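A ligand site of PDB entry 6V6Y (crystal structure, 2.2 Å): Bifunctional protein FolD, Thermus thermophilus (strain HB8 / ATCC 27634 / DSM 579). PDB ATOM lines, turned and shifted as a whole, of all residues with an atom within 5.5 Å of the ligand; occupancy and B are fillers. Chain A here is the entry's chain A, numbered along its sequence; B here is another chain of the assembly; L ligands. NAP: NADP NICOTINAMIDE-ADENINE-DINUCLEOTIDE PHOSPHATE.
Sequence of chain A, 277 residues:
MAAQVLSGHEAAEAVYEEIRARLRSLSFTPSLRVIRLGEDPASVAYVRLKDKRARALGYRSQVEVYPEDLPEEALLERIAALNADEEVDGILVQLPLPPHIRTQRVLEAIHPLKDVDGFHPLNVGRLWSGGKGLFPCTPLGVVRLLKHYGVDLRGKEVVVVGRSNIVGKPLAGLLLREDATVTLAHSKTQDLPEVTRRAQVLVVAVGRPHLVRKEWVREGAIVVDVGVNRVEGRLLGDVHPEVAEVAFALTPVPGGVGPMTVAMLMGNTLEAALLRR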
ATOM      1  N   TYR A  46      22.930 -44.396   6.897  1.00  0.00           N
ATOM      2  CA  TYR A  46      21.761 -43.896   6.172  1.00  0.00           C
ATOM      3  C   TYR A  46      21.172 -44.958   5.259  1.00  0.00           C
ATOM      4  O   TYR A  46      19.954 -45.205   5.270  1.00  0.00           O
ATOM      5  CB  TYR A  46      22.150 -42.661   5.354  1.00  0.00           C
ATOM      6  CG  TYR A  46      21.977 -41.369   6.100  1.00  0.00           C
ATOM      7  CD1 TYR A  46      20.947 -41.216   7.023  1.00  0.00           C
ATOM      8  CD2 TYR A  46      22.853 -40.300   5.895  1.00  0.00           C
ATOM      9  CE1 TYR A  46      20.783 -40.036   7.722  1.00  0.00           C
ATOM     10  CE2 TYR A  46      22.700 -39.107   6.597  1.00  0.00           C
ATOM     11  CZ  TYR A  46      21.658 -38.981   7.516  1.00  0.00           C
ATOM     12  OH  TYR A  46      21.482 -37.807   8.218  1.00  0.00           O
ATOM     13  N   THR A 138      13.394 -34.764   1.969  1.00  0.00           N
ATOM     14  CA  THR A 138      13.334 -33.966   3.191  1.00  0.00           C
ATOM     15  C   THR A 138      12.343 -32.813   3.053  1.00  0.00           C
ATOM     16  O   THR A 138      11.498 -32.654   3.941  1.00  0.00           O
ATOM     17  CB  THR A 138      14.720 -33.464   3.584  1.00  0.00           C
ATOM     18  OG1 THR A 138      15.592 -34.588   3.759  1.00  0.00           O
ATOM     19  CG2 THR A 138      14.654 -32.657   4.877  1.00  0.00           C
ATOM     20  N   VAL A 161      16.260 -21.331   6.400  1.00  0.00           N
ATOM     21  CA  VAL A 161      17.666 -20.981   6.513  1.00  0.00           C
ATOM     22  C   VAL A 161      18.497 -22.110   5.943  1.00  0.00           C
ATOM     23  O   VAL A 161      18.536 -23.215   6.500  1.00  0.00           O
ATOM     24  CB  VAL A 161      18.092 -20.663   7.952  1.00  0.00           C
ATOM     25  CG1 VAL A 161      19.510 -20.063   7.949  1.00  0.00           C
ATOM     26  CG2 VAL A 161      17.095 -19.690   8.627  1.00  0.00           C
ATOM     27  N   GLY A 162      19.202 -21.822   4.847  1.00  0.00           N
ATOM     28  CA  GLY A 162      19.953 -22.811   4.111  1.00  0.00           C
ATOM     29  C   GLY A 162      19.346 -22.933   2.741  1.00  0.00           C
ATOM     30  O   GLY A 162      18.118 -22.941   2.601  1.00  0.00           O
ATOM     31  N   ARG A 163      20.171 -23.017   1.713  1.00  0.00           N
ATOM     32  CA  ARG A 163      19.676 -22.950   0.350  1.00  0.00           C
ATOM     33  C   ARG A 163      20.234 -24.077  -0.506  1.00  0.00           C
ATOM     34  O   ARG A 163      20.554 -23.884  -1.678  1.00  0.00           O
ATOM     35  CB  ARG A 163      20.003 -21.588  -0.280  1.00  0.00           C
ATOM     36  CG  ARG A 163      21.481 -21.287  -0.276  1.00  0.00           C
ATOM     37  CD  ARG A 163      21.855 -20.103  -1.144  1.00  0.00           C
ATOM     38  NE  ARG A 163      23.212 -19.681  -0.792  1.00  0.00           N
ATOM     39  CZ  ARG A 163      23.880 -18.695  -1.373  1.00  0.00           C
ATOM     40  NH1 ARG A 163      23.323 -18.016  -2.377  1.00  0.00           N
ATOM     41  NH2 ARG A 163      25.095 -18.393  -0.959  1.00  0.00           N
ATOM     42  N   SER A 164      20.361 -25.276   0.068  1.00  0.00           N
ATOM     43  CA  SER A 164      20.921 -26.381  -0.698  1.00  0.00           C
ATOM     44  C   SER A 164      19.893 -26.950  -1.670  1.00  0.00           C
ATOM     45  O   SER A 164      18.691 -26.671  -1.576  1.00  0.00           O
ATOM     46  CB  SER A 164      21.395 -27.496   0.242  1.00  0.00           C
ATOM     47  OG  SER A 164      20.268 -28.250   0.642  1.00  0.00           O
ATOM     48  N   ILE A 166      19.381 -30.118  -1.725  1.00  0.00           N
ATOM     49  CA  ILE A 166      18.781 -31.248  -1.019  1.00  0.00           C
ATOM     50  C   ILE A 166      17.632 -30.805  -0.117  1.00  0.00           C
ATOM     51  O   ILE A 166      16.664 -31.543   0.061  1.00  0.00           O
ATOM     52  CB  ILE A 166      19.884 -31.993  -0.257  1.00  0.00           C
ATOM     53  CG1 ILE A 166      20.820 -32.657  -1.273  1.00  0.00           C
ATOM     54  CG2 ILE A 166      19.304 -33.059   0.705  1.00  0.00           C
ATOM     55  CD1 ILE A 166      22.246 -32.763  -0.800  1.00  0.00           C
ATOM     56  N   VAL A 167      17.699 -29.586   0.458  1.00  0.00           N
ATOM     57  CA  VAL A 167      16.650 -29.133   1.377  1.00  0.00           C
ATOM     58  C   VAL A 167      16.085 -27.754   1.027  1.00  0.00           C
ATOM     59  O   VAL A 167      14.923 -27.627   0.627  1.00  0.00           O
ATOM     60  CB  VAL A 167      17.170 -29.137   2.837  1.00  0.00           C
ATOM     61  CG1 VAL A 167      16.070 -28.731   3.778  1.00  0.00           C
ATOM     62  CG2 VAL A 167      17.742 -30.497   3.212  1.00  0.00           C
ATOM     63  N   HIS A 186      20.582 -17.651   4.226  1.00  0.00           N
ATOM     64  CA  HIS A 186      21.765 -18.471   3.968  1.00  0.00           C
ATOM     65  C   HIS A 186      22.962 -17.777   4.594  1.00  0.00           C
ATOM     66  O   HIS A 186      22.816 -16.777   5.310  1.00  0.00           O
ATOM     67  CB  HIS A 186      21.967 -18.677   2.462  1.00  0.00           C
ATOM     68  CG  HIS A 186      21.844 -17.413   1.681  1.00  0.00           C
ATOM     69  ND1 HIS A 186      22.769 -16.392   1.770  1.00  0.00           N
ATOM     70  CD2 HIS A 186      20.883 -16.973   0.836  1.00  0.00           C
ATOM     71  CE1 HIS A 186      22.405 -15.396   0.968  1.00  0.00           C
ATOM     72  NE2 HIS A 186      21.253 -15.721   0.408  1.00  0.00           N
ATOM     73  N   SER A 187      24.154 -18.290   4.304  1.00  0.00           N
ATOM     74  CA  SER A 187      25.322 -17.822   5.035  1.00  0.00           C
ATOM     75  C   SER A 187      25.698 -16.373   4.714  1.00  0.00           C
ATOM     76  O   SER A 187      26.472 -15.778   5.465  1.00  0.00           O
ATOM     77  CB  SER A 187      26.506 -18.748   4.766  1.00  0.00           C
ATOM     78  OG  SER A 187      27.085 -18.451   3.508  1.00  0.00           O
ATOM     79  N   LYS A 188      25.168 -15.784   3.646  1.00  0.00           N
ATOM     80  CA  LYS A 188      25.480 -14.399   3.305  1.00  0.00           C
ATOM     81  C   LYS A 188      24.369 -13.436   3.675  1.00  0.00           C
ATOM     82  O   LYS A 188      24.460 -12.232   3.358  1.00  0.00           O
ATOM     83  CB  LYS A 188      25.801 -14.260   1.802  1.00  0.00           C
ATOM     84  CG  LYS A 188      26.980 -15.100   1.332  1.00  0.00           C
ATOM     85  CD  LYS A 188      28.241 -14.654   2.055  1.00  0.00           C
ATOM     86  CE  LYS A 188      29.477 -14.975   1.232  1.00  0.00           C
ATOM     87  NZ  LYS A 188      29.651 -16.447   1.096  1.00  0.00           N
ATOM     88  N   LEU A 192      21.185 -12.185  10.280  1.00  0.00           N
ATOM     89  CA  LEU A 192      20.343 -13.380  10.239  1.00  0.00           C
ATOM     90  C   LEU A 192      19.329 -13.445  11.388  1.00  0.00           C
ATOM     91  O   LEU A 192      18.155 -13.739  11.109  1.00  0.00           O
ATOM     92  CB  LEU A 192      21.240 -14.622  10.255  1.00  0.00           C
ATOM     93  CG  LEU A 192      20.851 -15.850   9.426  1.00  0.00           C
ATOM     94  CD1 LEU A 192      21.325 -17.084  10.134  1.00  0.00           C
ATOM     95  CD2 LEU A 192      19.353 -15.919   9.087  1.00  0.00           C
ATOM     96  N   ALA A 205      18.180 -25.572   8.106  1.00  0.00           N
ATOM     97  CA  ALA A 205      18.992 -26.654   7.504  1.00  0.00           C
ATOM     98  C   ALA A 205      20.375 -26.098   7.156  1.00  0.00           C
ATOM     99  O   ALA A 205      20.708 -25.878   5.987  1.00  0.00           O
ATOM    100  CB  ALA A 205      18.301 -27.249   6.278  1.00  0.00           C
ATOM    101  N   VAL A 206      21.219 -25.913   8.165  1.00  0.00           N
ATOM    102  CA  VAL A 206      22.540 -25.340   7.955  1.00  0.00           C
ATOM    103  C   VAL A 206      23.682 -26.257   8.390  1.00  0.00           C
ATOM    104  O   VAL A 206      24.808 -26.094   7.900  1.00  0.00           O
ATOM    105  CB  VAL A 206      22.673 -23.973   8.663  1.00  0.00           C
ATOM    106  CG1 VAL A 206      21.637 -23.000   8.111  1.00  0.00           C
ATOM    107  CG2 VAL A 206      22.488 -24.144  10.146  1.00  0.00           C
ATOM    108  N   GLY A 207      23.448 -27.214   9.289  1.00  0.00           N
ATOM    109  CA  GLY A 207      24.532 -28.063   9.735  1.00  0.00           C
ATOM    110  C   GLY A 207      25.512 -27.409  10.692  1.00  0.00           C
ATOM    111  O   GLY A 207      26.716 -27.660  10.600  1.00  0.00           O
ATOM    112  N   ARG A 208      25.024 -26.571  11.600  1.00  0.00           N
ATOM    113  CA  ARG A 208      25.826 -25.967  12.672  1.00  0.00           C
ATOM    114  C   ARG A 208      25.100 -26.296  13.965  1.00  0.00           C
ATOM    115  O   ARG A 208      23.965 -25.839  14.164  1.00  0.00           O
ATOM    116  CB  ARG A 208      25.989 -24.452  12.491  1.00  0.00           C
ATOM    117  CG  ARG A 208      26.401 -23.958  11.072  1.00  0.00           C
ATOM    118  CD  ARG A 208      27.679 -24.623  10.526  1.00  0.00           C
ATOM    119  NE  ARG A 208      28.221 -23.992   9.313  1.00  0.00           N
ATOM    120  CZ  ARG A 208      28.477 -24.642   8.161  1.00  0.00           C
ATOM    121  NH1 ARG A 208      28.234 -25.959   8.070  1.00  0.00           N
ATOM    122  NH2 ARG A 208      28.973 -23.996   7.106  1.00  0.00           N
ATOM    123  N   LEU A 211      23.139 -23.699  16.558  1.00  0.00           N
ATOM    124  CA  LEU A 211      23.405 -22.336  16.096  1.00  0.00           C
ATOM    125  C   LEU A 211      22.276 -21.378  16.454  1.00  0.00           C
ATOM    126  O   LEU A 211      22.517 -20.285  16.977  1.00  0.00           O
ATOM    127  CB  LEU A 211      23.658 -22.375  14.582  1.00  0.00           C
ATOM    128  CG  LEU A 211      24.152 -21.224  13.719  1.00  0.00           C
ATOM    129  CD1 LEU A 211      22.997 -20.435  13.195  1.00  0.00           C
ATOM    130  CD2 LEU A 211      25.051 -20.338  14.509  1.00  0.00           C
ATOM    131  N   VAL A 226      16.177 -29.259  10.736  1.00  0.00           N
ATOM    132  CA  VAL A 226      16.653 -30.286   9.793  1.00  0.00           C
ATOM    133  C   VAL A 226      18.078 -30.727  10.080  1.00  0.00           C
ATOM    134  O   VAL A 226      18.515 -31.760   9.558  1.00  0.00           O
ATOM    135  CB  VAL A 226      16.517 -29.754   8.344  1.00  0.00           C
ATOM    136  CG1 VAL A 226      16.792 -30.835   7.313  1.00  0.00           C
ATOM    137  CG2 VAL A 226      15.116 -29.163   8.114  1.00  0.00           C
ATOM    138  N   GLY A 227      18.807 -30.009  10.944  1.00  0.00           N
ATOM    139  CA  GLY A 227      20.203 -30.326  11.143  1.00  0.00           C
ATOM    140  C   GLY A 227      20.399 -31.687  11.791  1.00  0.00           C
ATOM    141  O   GLY A 227      19.588 -32.144  12.605  1.00  0.00           O
ATOM    142  N   VAL A 228      21.482 -32.348  11.416  1.00  0.00           N
ATOM    143  CA  VAL A 228      21.865 -33.604  12.063  1.00  0.00           C
ATOM    144  C   VAL A 228      23.370 -33.528  12.288  1.00  0.00           C
ATOM    145  O   VAL A 228      24.161 -33.845  11.385  1.00  0.00           O
ATOM    146  CB  VAL A 228      21.470 -34.830  11.219  1.00  0.00           C
ATOM    147  CG1 VAL A 228      22.177 -36.084  11.720  1.00  0.00           C
ATOM    148  CG2 VAL A 228      19.954 -35.021  11.204  1.00  0.00           C
ATOM    149  N   ASN A 229      23.794 -33.068  13.450  1.00  0.00           N
ATOM    150  CA  ASN A 229      25.206 -32.801  13.720  1.00  0.00           C
ATOM    151  C   ASN A 229      25.735 -33.840  14.720  1.00  0.00           C
ATOM    152  O   ASN A 229      25.362 -33.816  15.906  1.00  0.00           O
ATOM    153  CB  ASN A 229      25.401 -31.376  14.234  1.00  0.00           C
ATOM    154  CG  ASN A 229      24.803 -30.329  13.312  1.00  0.00           C
ATOM    155  OD1 ASN A 229      25.393 -29.979  12.293  1.00  0.00           O
ATOM    156  ND2 ASN A 229      23.616 -29.842  13.653  1.00  0.00           N
ATOM    157  N   ASP A 238      20.389 -28.146  14.471  1.00  0.00           N
ATOM    158  CA  ASP A 238      20.911 -26.798  14.274  1.00  0.00           C
ATOM    159  C   ASP A 238      20.296 -25.802  15.225  1.00  0.00           C
ATOM    160  O   ASP A 238      20.748 -24.650  15.278  1.00  0.00           O
ATOM    161  CB  ASP A 238      20.662 -26.301  12.855  1.00  0.00           C
ATOM    162  CG  ASP A 238      21.311 -27.159  11.824  1.00  0.00           C
ATOM    163  OD1 ASP A 238      22.383 -27.731  12.100  1.00  0.00           O
ATOM    164  OD2 ASP A 238      20.738 -27.240  10.719  1.00  0.00           O
ATOM    165  N   VAL A 257      12.611 -34.420  11.889  1.00  0.00           N
ATOM    166  CA  VAL A 257      12.593 -34.446  10.433  1.00  0.00           C
ATOM    167  C   VAL A 257      13.061 -35.795   9.901  1.00  0.00           C
ATOM    168  O   VAL A 257      12.502 -36.321   8.929  1.00  0.00           O
ATOM    169  CB  VAL A 257      13.464 -33.296   9.895  1.00  0.00           C
ATOM    170  CG1 VAL A 257      13.690 -33.469   8.389  1.00  0.00           C
ATOM    171  CG2 VAL A 257      12.838 -31.957  10.264  1.00  0.00           C
ATOM    172  N   GLY A 258      14.083 -36.373  10.514  1.00  0.00           N
ATOM    173  CA  GLY A 258      14.722 -37.576  10.024  1.00  0.00           C
ATOM    174  C   GLY A 258      13.769 -38.688   9.662  1.00  0.00           C
ATOM    175  O   GLY A 258      13.835 -39.261   8.562  1.00  0.00           O
ATOM    176  N   THR A 261      11.949 -37.840   6.442  1.00  0.00           N
ATOM    177  CA  THR A 261      12.735 -38.013   5.233  1.00  0.00           C
ATOM    178  C   THR A 261      12.676 -39.460   4.743  1.00  0.00           C
ATOM    179  O   THR A 261      12.575 -39.710   3.532  1.00  0.00           O
ATOM    180  CB  THR A 261      14.196 -37.621   5.478  1.00  0.00           C
ATOM    181  OG1 THR A 261      14.275 -36.243   5.896  1.00  0.00           O
ATOM    182  CG2 THR A 261      15.025 -37.813   4.169  1.00  0.00           C
ATOM    183  N   ASP B 179      23.622 -14.157  -4.196  1.00  0.00           N
ATOM    184  CA  ASP B 179      23.764 -14.148  -2.747  1.00  0.00           C
ATOM    185  C   ASP B 179      22.877 -13.115  -2.071  1.00  0.00           C
ATOM    186  O   ASP B 179      23.180 -12.654  -0.968  1.00  0.00           O
ATOM    187  CB  ASP B 179      25.220 -13.955  -2.309  1.00  0.00           C
ATOM    188  CG  ASP B 179      26.097 -15.170  -2.632  1.00  0.00           C
ATOM    189  OD1 ASP B 179      25.539 -16.270  -2.869  1.00  0.00           O
ATOM    190  OD2 ASP B 179      27.332 -15.025  -2.630  1.00  0.00           O
HETATM  191  PA  NAP L   1      24.538 -27.565   2.767  1.00  0.00           P
HETATM  192  O1A NAP L   1      25.613 -28.485   3.221  1.00  0.00           O
HETATM  193  O2A NAP L   1      24.564 -27.395   1.302  1.00  0.00           O
HETATM  194  O5B NAP L   1      24.674 -26.152   3.528  1.00  0.00           O
HETATM  195  C5B NAP L   1      23.579 -25.667   4.264  1.00  0.00           C
HETATM  196  C4B NAP L   1      23.375 -24.178   4.014  1.00  0.00           C
HETATM  197  O4B NAP L   1      23.293 -23.478   5.240  1.00  0.00           O
HETATM  198  C3B NAP L   1      24.502 -23.537   3.214  1.00  0.00           C
HETATM  199  O3B NAP L   1      24.094 -23.387   1.869  1.00  0.00           O
HETATM  200  C2B NAP L   1      24.785 -22.209   3.883  1.00  0.00           C
HETATM  201  O2B NAP L   1      24.444 -21.101   3.078  1.00  0.00           O
HETATM  202  C1B NAP L   1      23.908 -22.215   5.134  1.00  0.00           C
HETATM  203  N9A NAP L   1      24.720 -21.914   6.331  1.00  0.00           N
HETATM  204  C8A NAP L   1      25.748 -22.683   6.833  1.00  0.00           C
HETATM  205  N7A NAP L   1      26.235 -22.067   7.931  1.00  0.00           N
HETATM  206  C5A NAP L   1      25.540 -20.932   8.148  1.00  0.00           C
HETATM  207  C6A NAP L   1      25.628 -19.952   9.131  1.00  0.00           C
HETATM  208  N6A NAP L   1      26.546 -20.048  10.093  1.00  0.00           N
HETATM  209  N1A NAP L   1      24.770 -18.875   9.095  1.00  0.00           N
HETATM  210  C2A NAP L   1      23.819 -18.788   8.095  1.00  0.00           C
HETATM  211  N3A NAP L   1      23.737 -19.770   7.128  1.00  0.00           N
HETATM  212  C4A NAP L   1      24.581 -20.815   7.148  1.00  0.00           C
HETATM  213  O3  NAP L   1      23.110 -28.114   3.265  1.00  0.00           O
HETATM  214  PN  NAP L   1      22.542 -29.597   3.509  1.00  0.00           P
HETATM  215  O1N NAP L   1      23.158 -30.497   2.512  1.00  0.00           O
HETATM  216  O2N NAP L   1      21.074 -29.524   3.629  1.00  0.00           O
HETATM  217  O5D NAP L   1      23.164 -29.944   4.954  1.00  0.00           O
HETATM  218  C5D NAP L   1      22.781 -29.181   6.081  1.00  0.00           C
HETATM  219  C4D NAP L   1      22.515 -30.078   7.274  1.00  0.00           C
HETATM  220  O4D NAP L   1      21.266 -30.739   7.140  1.00  0.00           O
HETATM  221  C3D NAP L   1      23.579 -31.158   7.397  1.00  0.00           C
HETATM  222  O3D NAP L   1      24.170 -31.098   8.673  1.00  0.00           O
HETATM  223  C2D NAP L   1      22.847 -32.468   7.231  1.00  0.00           C
HETATM  224  O2D NAP L   1      23.285 -33.396   8.186  1.00  0.00           O
HETATM  225  C1D NAP L   1      21.392 -32.106   7.471  1.00  0.00           C
HETATM  226  N1N NAP L   1      20.507 -32.948   6.644  1.00  0.00           N
HETATM  227  C2N NAP L   1      19.582 -33.737   7.267  1.00  0.00           C
HETATM  228  C3N NAP L   1      18.732 -34.546   6.523  1.00  0.00           C
HETATM  229  C7N NAP L   1      17.657 -35.326   7.212  1.00  0.00           C
HETATM  230  O7N NAP L   1      16.871 -36.225   6.464  1.00  0.00           O
HETATM  231  N7N NAP L   1      17.461 -35.133   8.515  1.00  0.00           N
HETATM  232  C4N NAP L   1      18.823 -34.545   5.139  1.00  0.00           C
HETATM  233  C5N NAP L   1      19.771 -33.737   4.515  1.00  0.00           C
HETATM  234  C6N NAP L   1      20.614 -32.943   5.286  1.00  0.00           C
HETATM  235  P2B NAP L   1      25.339 -20.662   1.817  1.00  0.00           P
HETATM  236  O1X NAP L   1      25.046 -21.567   0.643  1.00  0.00           O
HETATM  237  O2X NAP L   1      24.999 -19.245   1.451  1.00  0.00           O
HETATM  238  O3X NAP L   1      26.805 -20.762   2.169  1.00  0.00           O
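O3X of the ligand sits at hydrogen-bond distance from OG of Ser 187. NE of Arg 208 is in hydrogen-bond range of N7A of the ligand (3.1 Å). NH2 of Arg 163 is in salt-bridge range of O2X of the ligand (2.6 Å). OG1 of Thr 261 is in hydrogen-bond range of O7N of the ligand, 2.7 Å away. The backbone carbonyl oxygen (O) of Val 228 lies within hydrogen-bond range of an oxygen (O2D) of the ligand (3.3 Å). An oxygen (O7N) of the ligand is in hydrogen-bond range of the side-chain hydroxyl (OG1) of Thr 138 (3.4 Å). The side-chain hydroxyl (OG) of Ser 164 lies within hydrogen-bond range of an oxygen (O2N) of the ligand. The backbone NH (N) of Ser 187 lies within hydrogen-bond range of an oxygen (O2B) of the ligand (3.1 Å).
The backbone NH (N) of Arg 208 sits at hydrogen-bond distance from the side-chain amide oxygen (OD1) of Asn 229 (3.5 Å). The backbone NH of Val 167 sits at hydrogen-bond distance from the side-chain hydroxyl of Ser 164 (2.9 Å). O of Val 161 is in hydrogen-bond range of N of Ala 205, at 2.9 Å. The backbone NH (N) of Gly 207 is in hydrogen-bond range of the side-chain carboxylate (OD1) of Asp 238, at 3.1 Å. OG1 of Thr 261 lies within hydrogen-bond range of OG1 of Thr 138 (3.0 Å). N of Arg 208 is in hydrogen-bond range of OD1 of Asp 238, 2.9 Å away. OD2 of Asp 238 is in hydrogen-bond range of N of Val 206 (2.9 Å). The backbone carbonyl oxygen (O) of Val 206 sits at hydrogen-bond distance from the guanidinium group (NH1) of Arg 208, 3.4 Å away.
Gly 162 touches the ligand (CA to O4B, 3.6 Å). Ile 166 touches the ligand. Val 167 touches the ligand (CG2 to O2N, 3.5 Å). His 186 touches the ligand (CB to O2X, 3.2 Å). Leu 192 touches the ligand. O of Ala 205 touches C5B of the ligand, at 3.4 Å. Val 206 touches the ligand (CG1 to O4B, 3.3 Å). Gly 207 touches the ligand (CA to O3D, 3.2 Å). O of Val 226 touches C2N of the ligand (3.2 Å). Asn 229 touches the ligand (OD1 to O3D, 3.98 Å). Gly 258 touches the ligand. 18 residues have an atom within 4 Å of the ligand: Thr 138, Gly 162, Arg 163, Ser 164, Ile 166, Val 167, His 186, Ser 187, Leu 192, Ala 205, Val 206, Gly 207, Arg 208, Val 226, Val 228, Asn 229, Gly 258 and Thr 261.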
